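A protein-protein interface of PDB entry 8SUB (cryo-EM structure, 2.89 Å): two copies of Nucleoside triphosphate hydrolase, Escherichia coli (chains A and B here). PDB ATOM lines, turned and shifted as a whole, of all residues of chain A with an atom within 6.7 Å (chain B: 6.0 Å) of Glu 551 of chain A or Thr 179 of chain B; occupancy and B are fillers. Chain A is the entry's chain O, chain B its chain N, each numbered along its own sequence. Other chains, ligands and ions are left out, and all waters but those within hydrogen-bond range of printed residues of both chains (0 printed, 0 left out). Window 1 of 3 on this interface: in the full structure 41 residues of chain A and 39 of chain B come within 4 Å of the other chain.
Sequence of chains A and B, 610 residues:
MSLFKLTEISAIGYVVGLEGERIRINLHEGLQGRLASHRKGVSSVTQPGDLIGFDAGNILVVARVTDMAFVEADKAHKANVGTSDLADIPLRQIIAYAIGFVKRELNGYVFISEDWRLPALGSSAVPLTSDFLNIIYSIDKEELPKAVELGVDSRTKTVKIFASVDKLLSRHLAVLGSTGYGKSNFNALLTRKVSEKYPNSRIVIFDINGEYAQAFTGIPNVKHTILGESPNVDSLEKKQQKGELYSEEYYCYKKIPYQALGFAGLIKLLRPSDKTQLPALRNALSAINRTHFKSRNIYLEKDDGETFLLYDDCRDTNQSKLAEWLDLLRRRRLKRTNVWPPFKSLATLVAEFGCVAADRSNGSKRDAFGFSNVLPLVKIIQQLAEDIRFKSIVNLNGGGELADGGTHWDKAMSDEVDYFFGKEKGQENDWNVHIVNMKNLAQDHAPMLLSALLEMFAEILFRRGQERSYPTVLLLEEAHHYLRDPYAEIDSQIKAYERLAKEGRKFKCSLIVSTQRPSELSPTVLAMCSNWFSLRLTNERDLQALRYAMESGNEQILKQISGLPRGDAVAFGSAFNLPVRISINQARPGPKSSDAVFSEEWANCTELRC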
ATOM      1  N   ARG A 171       0.343  13.475  12.509  1.00  0.00           N
ATOM      2  CA  ARG A 171      -0.109  14.169  13.707  1.00  0.00           C
ATOM      3  C   ARG A 171       0.029  13.237  14.905  1.00  0.00           C
ATOM      4  O   ARG A 171       0.521  12.115  14.792  1.00  0.00           O
ATOM      5  CB  ARG A 171      -1.550  14.658  13.554  1.00  0.00           C
ATOM      6  CG  ARG A 171      -1.675  16.050  12.968  1.00  0.00           C
ATOM      7  CD  ARG A 171      -1.383  16.030  11.486  1.00  0.00           C
ATOM      8  NE  ARG A 171      -2.233  15.072  10.793  1.00  0.00           N
ATOM      9  CZ  ARG A 171      -3.443  15.345  10.324  1.00  0.00           C
ATOM     10  NH1 ARG A 171      -3.970  16.554  10.439  1.00  0.00           N
ATOM     11  NH2 ARG A 171      -4.140  14.382   9.729  1.00  0.00           N
ATOM     12  N   ALA A 527      -6.008  17.119  23.956  1.00  0.00           N
ATOM     13  CA  ALA A 527      -6.738  17.851  22.930  1.00  0.00           C
ATOM     14  C   ALA A 527      -5.890  18.171  21.706  1.00  0.00           C
ATOM     15  O   ALA A 527      -6.386  18.823  20.784  1.00  0.00           O
ATOM     16  CB  ALA A 527      -7.304  19.145  23.513  1.00  0.00           C
ATOM     17  N   CYS A 529      -4.370  15.624  19.973  1.00  0.00           N
ATOM     18  CA  CYS A 529      -4.356  14.410  19.175  1.00  0.00           C
ATOM     19  C   CYS A 529      -5.433  14.455  18.102  1.00  0.00           C
ATOM     20  O   CYS A 529      -6.496  15.048  18.286  1.00  0.00           O
ATOM     21  CB  CYS A 529      -4.554  13.179  20.062  1.00  0.00           C
ATOM     22  SG  CYS A 529      -3.406  13.059  21.447  1.00  0.00           S
ATOM     23  N   TRP A 532      -7.856   8.635  17.787  1.00  0.00           N
ATOM     24  CA  TRP A 532      -8.000   7.992  19.083  1.00  0.00           C
ATOM     25  C   TRP A 532      -8.227   6.502  18.892  1.00  0.00           C
ATOM     26  O   TRP A 532      -9.078   6.101  18.096  1.00  0.00           O
ATOM     27  CB  TRP A 532      -9.163   8.592  19.885  1.00  0.00           C
ATOM     28  CG  TRP A 532      -8.926   9.989  20.387  1.00  0.00           C
ATOM     29  CD1 TRP A 532      -8.419  10.346  21.598  1.00  0.00           C
ATOM     30  CD2 TRP A 532      -9.208  11.212  19.698  1.00  0.00           C
ATOM     31  NE1 TRP A 532      -8.351  11.709  21.702  1.00  0.00           N
ATOM     32  CE2 TRP A 532      -8.832  12.265  20.549  1.00  0.00           C
ATOM     33  CE3 TRP A 532      -9.737  11.517  18.443  1.00  0.00           C
ATOM     34  CZ2 TRP A 532      -8.967  13.599  20.186  1.00  0.00           C
ATOM     35  CZ3 TRP A 532      -9.871  12.841  18.084  1.00  0.00           C
ATOM     36  CH2 TRP A 532      -9.488  13.866  18.951  1.00  0.00           C
ATOM     37  N   LEU A 546     -12.571  11.630  28.607  1.00  0.00           N
ATOM     38  CA  LEU A 546     -12.510  11.438  27.167  1.00  0.00           C
ATOM     39  C   LEU A 546     -13.708  12.043  26.452  1.00  0.00           C
ATOM     40  O   LEU A 546     -13.569  12.523  25.324  1.00  0.00           O
ATOM     41  CB  LEU A 546     -12.398   9.947  26.847  1.00  0.00           C
ATOM     42  CG  LEU A 546     -12.452   9.515  25.385  1.00  0.00           C
ATOM     43  CD1 LEU A 546     -11.300  10.116  24.605  1.00  0.00           C
ATOM     44  CD2 LEU A 546     -12.417   8.006  25.299  1.00  0.00           C
ATOM     45  N   ALA A 549     -12.890  15.914  25.568  1.00  0.00           N
ATOM     46  CA  ALA A 549     -11.827  16.392  24.696  1.00  0.00           C
ATOM     47  C   ALA A 549     -11.887  15.879  23.263  1.00  0.00           C
ATOM     48  O   ALA A 549     -11.125  16.373  22.424  1.00  0.00           O
ATOM     49  CB  ALA A 549     -10.456  16.035  25.284  1.00  0.00           C
ATOM     50  N   MET A 550     -12.747  14.916  22.951  1.00  0.00           N
ATOM     51  CA  MET A 550     -12.830  14.412  21.589  1.00  0.00           C
ATOM     52  C   MET A 550     -13.537  15.415  20.682  1.00  0.00           C
ATOM     53  O   MET A 550     -14.302  16.269  21.134  1.00  0.00           O
ATOM     54  CB  MET A 550     -13.552  13.068  21.558  1.00  0.00           C
ATOM     55  CG  MET A 550     -14.866  13.054  22.299  1.00  0.00           C
ATOM     56  SD  MET A 550     -15.904  11.676  21.812  1.00  0.00           S
ATOM     57  CE  MET A 550     -17.024  12.503  20.701  1.00  0.00           C
ATOM     58  N   GLU A 551     -13.271  15.302  19.381  1.00  0.00           N
ATOM     59  CA  GLU A 551     -13.892  16.183  18.397  1.00  0.00           C
ATOM     60  C   GLU A 551     -14.665  15.461  17.306  1.00  0.00           C
ATOM     61  O   GLU A 551     -15.612  16.029  16.767  1.00  0.00           O
ATOM     62  CB  GLU A 551     -12.849  17.081  17.724  1.00  0.00           C
ATOM     63  CG  GLU A 551     -12.215  18.099  18.637  1.00  0.00           C
ATOM     64  CD  GLU A 551     -11.183  18.950  17.923  1.00  0.00           C
ATOM     65  OE1 GLU A 551     -10.880  18.660  16.747  1.00  0.00           O
ATOM     66  OE2 GLU A 551     -10.671  19.907  18.539  1.00  0.00           O
ATOM     67  N   SER A 552     -14.292  14.238  16.949  1.00  0.00           N
ATOM     68  CA  SER A 552     -14.810  13.612  15.739  1.00  0.00           C
ATOM     69  C   SER A 552     -15.540  12.307  16.026  1.00  0.00           C
ATOM     70  O   SER A 552     -15.448  11.347  15.260  1.00  0.00           O
ATOM     71  CB  SER A 552     -13.687  13.379  14.735  1.00  0.00           C
ATOM     72  OG  SER A 552     -12.541  12.865  15.382  1.00  0.00           O
ATOM     73  N   GLY A 553     -16.308  12.260  17.106  1.00  0.00           N
ATOM     74  CA  GLY A 553     -17.040  11.053  17.421  1.00  0.00           C
ATOM     75  C   GLY A 553     -18.537  11.257  17.473  1.00  0.00           C
ATOM     76  O   GLY A 553     -19.069  12.153  16.815  1.00  0.00           O
ATOM     77  N   PHE A 572     -11.638   6.214  15.806  1.00  0.00           N
ATOM     78  CA  PHE A 572     -12.212   7.340  15.086  1.00  0.00           C
ATOM     79  C   PHE A 572     -11.182   8.456  15.018  1.00  0.00           C
ATOM     80  O   PHE A 572     -10.217   8.479  15.781  1.00  0.00           O
ATOM     81  CB  PHE A 572     -13.516   7.835  15.728  1.00  0.00           C
ATOM     82  CG  PHE A 572     -13.416   8.105  17.202  1.00  0.00           C
ATOM     83  CD1 PHE A 572     -13.654   7.102  18.115  1.00  0.00           C
ATOM     84  CD2 PHE A 572     -13.096   9.362  17.673  1.00  0.00           C
ATOM     85  CE1 PHE A 572     -13.567   7.344  19.463  1.00  0.00           C
ATOM     86  CE2 PHE A 572     -13.012   9.606  19.020  1.00  0.00           C
ATOM     87  CZ  PHE A 572     -13.244   8.596  19.914  1.00  0.00           C
ATOM     88  N   GLY B 177     -16.771  26.133  13.364  1.00  0.00           N
ATOM     89  CA  GLY B 177     -16.741  24.793  12.812  1.00  0.00           C
ATOM     90  C   GLY B 177     -15.527  24.031  13.281  1.00  0.00           C
ATOM     91  O   GLY B 177     -14.621  24.575  13.902  1.00  0.00           O
ATOM     92  N   SER B 178     -15.512  22.744  12.948  1.00  0.00           N
ATOM     93  CA  SER B 178     -14.425  21.856  13.341  1.00  0.00           C
ATOM     94  C   SER B 178     -13.204  22.093  12.455  1.00  0.00           C
ATOM     95  O   SER B 178     -13.093  23.106  11.762  1.00  0.00           O
ATOM     96  CB  SER B 178     -14.880  20.404  13.285  1.00  0.00           C
ATOM     97  OG  SER B 178     -15.658  20.071  14.416  1.00  0.00           O
ATOM     98  N   THR B 179     -12.256  21.161  12.483  1.00  0.00           N
ATOM     99  CA  THR B 179     -11.022  21.295  11.718  1.00  0.00           C
ATOM    100  C   THR B 179     -11.062  20.413  10.476  1.00  0.00           C
ATOM    101  O   THR B 179     -11.544  19.278  10.523  1.00  0.00           O
ATOM    102  CB  THR B 179      -9.810  20.954  12.587  1.00  0.00           C
ATOM    103  OG1 THR B 179      -8.612  21.136  11.827  1.00  0.00           O
ATOM    104  CG2 THR B 179      -9.877  19.530  13.088  1.00  0.00           C
ATOM    105  N   GLY B 180     -10.562  20.944   9.365  1.00  0.00           N
ATOM    106  CA  GLY B 180     -10.603  20.243   8.100  1.00  0.00           C
ATOM    107  C   GLY B 180     -11.900  20.350   7.334  1.00  0.00           C
ATOM    108  O   GLY B 180     -12.125  19.547   6.424  1.00  0.00           O
ATOM    109  N   TYR B 181     -12.760  21.316   7.660  1.00  0.00           N
ATOM    110  CA  TYR B 181     -14.065  21.425   7.022  1.00  0.00           C
ATOM    111  C   TYR B 181     -14.261  22.700   6.215  1.00  0.00           C
ATOM    112  O   TYR B 181     -15.234  22.780   5.460  1.00  0.00           O
ATOM    113  CB  TYR B 181     -15.181  21.299   8.068  1.00  0.00           C
ATOM    114  CG  TYR B 181     -15.514  19.865   8.407  1.00  0.00           C
ATOM    115  CD1 TYR B 181     -16.380  19.124   7.620  1.00  0.00           C
ATOM    116  CD2 TYR B 181     -14.938  19.245   9.501  1.00  0.00           C
ATOM    117  CE1 TYR B 181     -16.669  17.810   7.924  1.00  0.00           C
ATOM    118  CE2 TYR B 181     -15.218  17.937   9.809  1.00  0.00           C
ATOM    119  CZ  TYR B 181     -16.084  17.225   9.020  1.00  0.00           C
ATOM    120  OH  TYR B 181     -16.362  15.920   9.333  1.00  0.00           O
ATOM    121  N   GLY B 182     -13.375  23.688   6.327  1.00  0.00           N
ATOM    122  CA  GLY B 182     -13.424  24.797   5.391  1.00  0.00           C
ATOM    123  C   GLY B 182     -13.581  26.216   5.895  1.00  0.00           C
ATOM    124  O   GLY B 182     -14.205  27.031   5.215  1.00  0.00           O
ATOM    125  N   LYS B 183     -13.029  26.545   7.063  1.00  0.00           N
ATOM    126  CA  LYS B 183     -13.103  27.919   7.551  1.00  0.00           C
ATOM    127  C   LYS B 183     -12.200  28.851   6.746  1.00  0.00           C
ATOM    128  O   LYS B 183     -12.599  29.969   6.390  1.00  0.00           O
ATOM    129  CB  LYS B 183     -12.739  27.967   9.032  1.00  0.00           C
ATOM    130  CG  LYS B 183     -13.682  27.201   9.938  1.00  0.00           C
ATOM    131  CD  LYS B 183     -13.352  27.443  11.394  1.00  0.00           C
ATOM    132  CE  LYS B 183     -12.082  26.732  11.797  1.00  0.00           C
ATOM    133  NZ  LYS B 183     -12.218  25.261  11.705  1.00  0.00           N
ATOM    134  N   GLN B 516     -12.633  27.017  16.470  1.00  0.00           N
ATOM    135  CA  GLN B 516     -13.201  25.681  16.481  1.00  0.00           C
ATOM    136  C   GLN B 516     -13.755  25.280  17.836  1.00  0.00           C
ATOM    137  O   GLN B 516     -14.361  24.211  17.947  1.00  0.00           O
ATOM    138  CB  GLN B 516     -12.155  24.652  16.048  1.00  0.00           C
ATOM    139  CG  GLN B 516     -10.897  24.699  16.879  1.00  0.00           C
ATOM    140  CD  GLN B 516      -9.924  23.623  16.500  1.00  0.00           C
ATOM    141  OE1 GLN B 516     -10.227  22.766  15.680  1.00  0.00           O
ATOM    142  NE2 GLN B 516      -8.739  23.665  17.086  1.00  0.00           N
ATOM    143  N   ARG B 517     -13.566  26.103  18.860  1.00  0.00           N
ATOM    144  CA  ARG B 517     -14.081  25.845  20.200  1.00  0.00           C
ATOM    145  C   ARG B 517     -14.825  27.083  20.673  1.00  0.00           C
ATOM    146  O   ARG B 517     -14.296  27.876  21.461  1.00  0.00           O
ATOM    147  CB  ARG B 517     -12.957  25.459  21.160  1.00  0.00           C
ATOM    148  CG  ARG B 517     -12.458  24.046  20.955  1.00  0.00           C
ATOM    149  CD  ARG B 517     -13.529  23.065  21.393  1.00  0.00           C
ATOM    150  NE  ARG B 517     -13.204  21.682  21.071  1.00  0.00           N
ATOM    151  CZ  ARG B 517     -12.729  20.801  21.938  1.00  0.00           C
ATOM    152  NH1 ARG B 517     -12.458  21.136  23.187  1.00  0.00           N
ATOM    153  NH2 ARG B 517     -12.522  19.551  21.541  1.00  0.00           N
ATOM    154  N   THR B 538     -19.520  18.999  16.353  1.00  0.00           N
ATOM    155  CA  THR B 538     -19.824  17.657  16.842  1.00  0.00           C
ATOM    156  C   THR B 538     -20.006  17.569  18.351  1.00  0.00           C
ATOM    157  O   THR B 538     -20.964  16.949  18.819  1.00  0.00           O
ATOM    158  CB  THR B 538     -18.721  16.686  16.408  1.00  0.00           C
ATOM    159  OG1 THR B 538     -18.364  16.933  15.043  1.00  0.00           O
ATOM    160  CG2 THR B 538     -19.216  15.270  16.525  1.00  0.00           C
ATOM    161  N   ASN B 539     -19.093  18.141  19.128  1.00  0.00           N
ATOM    162  CA  ASN B 539     -19.181  18.067  20.580  1.00  0.00           C
ATOM    163  C   ASN B 539     -20.417  18.807  21.077  1.00  0.00           C
ATOM    164  O   ASN B 539     -20.722  19.906  20.611  1.00  0.00           O
ATOM    165  CB  ASN B 539     -17.918  18.667  21.196  1.00  0.00           C
ATOM    166  CG  ASN B 539     -17.515  17.997  22.493  1.00  0.00           C
ATOM    167  OD1 ASN B 539     -18.295  17.268  23.102  1.00  0.00           O
ATOM    168  ND2 ASN B 539     -16.288  18.243  22.924  1.00  0.00           N
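O of Glu 551 of chain A sits close to OG1 of Thr 538 of chain B (3.4 Å). NH2 of Arg 517 of chain B is in salt-bridge range of OE2 of Glu 551 of chain A (3.5 Å). The side-chain amide nitrogen (ND2) of Asn 539 of chain B sits at hydrogen-bond distance from the backbone carbonyl oxygen (O) of Met 550 of chain A (3.3 Å).
Ala 549 of chain A touches Arg 517 of chain B. Arg 517 of chain B touches Met 550 of chain A. OE1 of Glu 551 of chain A touches CG2 of Thr 179 of chain B, at 3.9 Å. Gly 553 of chain A touches Thr 538 of chain B.
Of the printed residues of chain B, Met 550 of chain A touches Arg 517 (3.8 Å) and Asn 539 (3.3 Å). Of the printed residues of chain B, Glu 551 of chain A touches Thr 179, Arg 517 and Thr 538. Gly 177 of chain B touches none of the printed residues of chain A. Gly 182 of chain B touches none of the printed residues of chain A. Of the printed residues of chain A, Arg 517 of chain B touches Ala 549 (3.6 Å), Met 550 (3.8 Å) and Glu 551 (3.3 Å). Printed residues of chain A within 4 Å of Asn 539 of chain B: Met 550 (3.3 Å). The nearest printed residue of chain A that does not touch Thr 179 of chain B is Arg 171 of chain A (6.7 Å). The nearest printed residue of chain A that does not touch Thr 538 of chain B is Ser 552 of chain A (4.7 Å).
Of the 11 printed residues of chain A, 4 touch a printed residue of chain B. Along chain A the printed residues that touch a printed residue of chain B span positions 549 to 553.
No position is printed for both chains.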
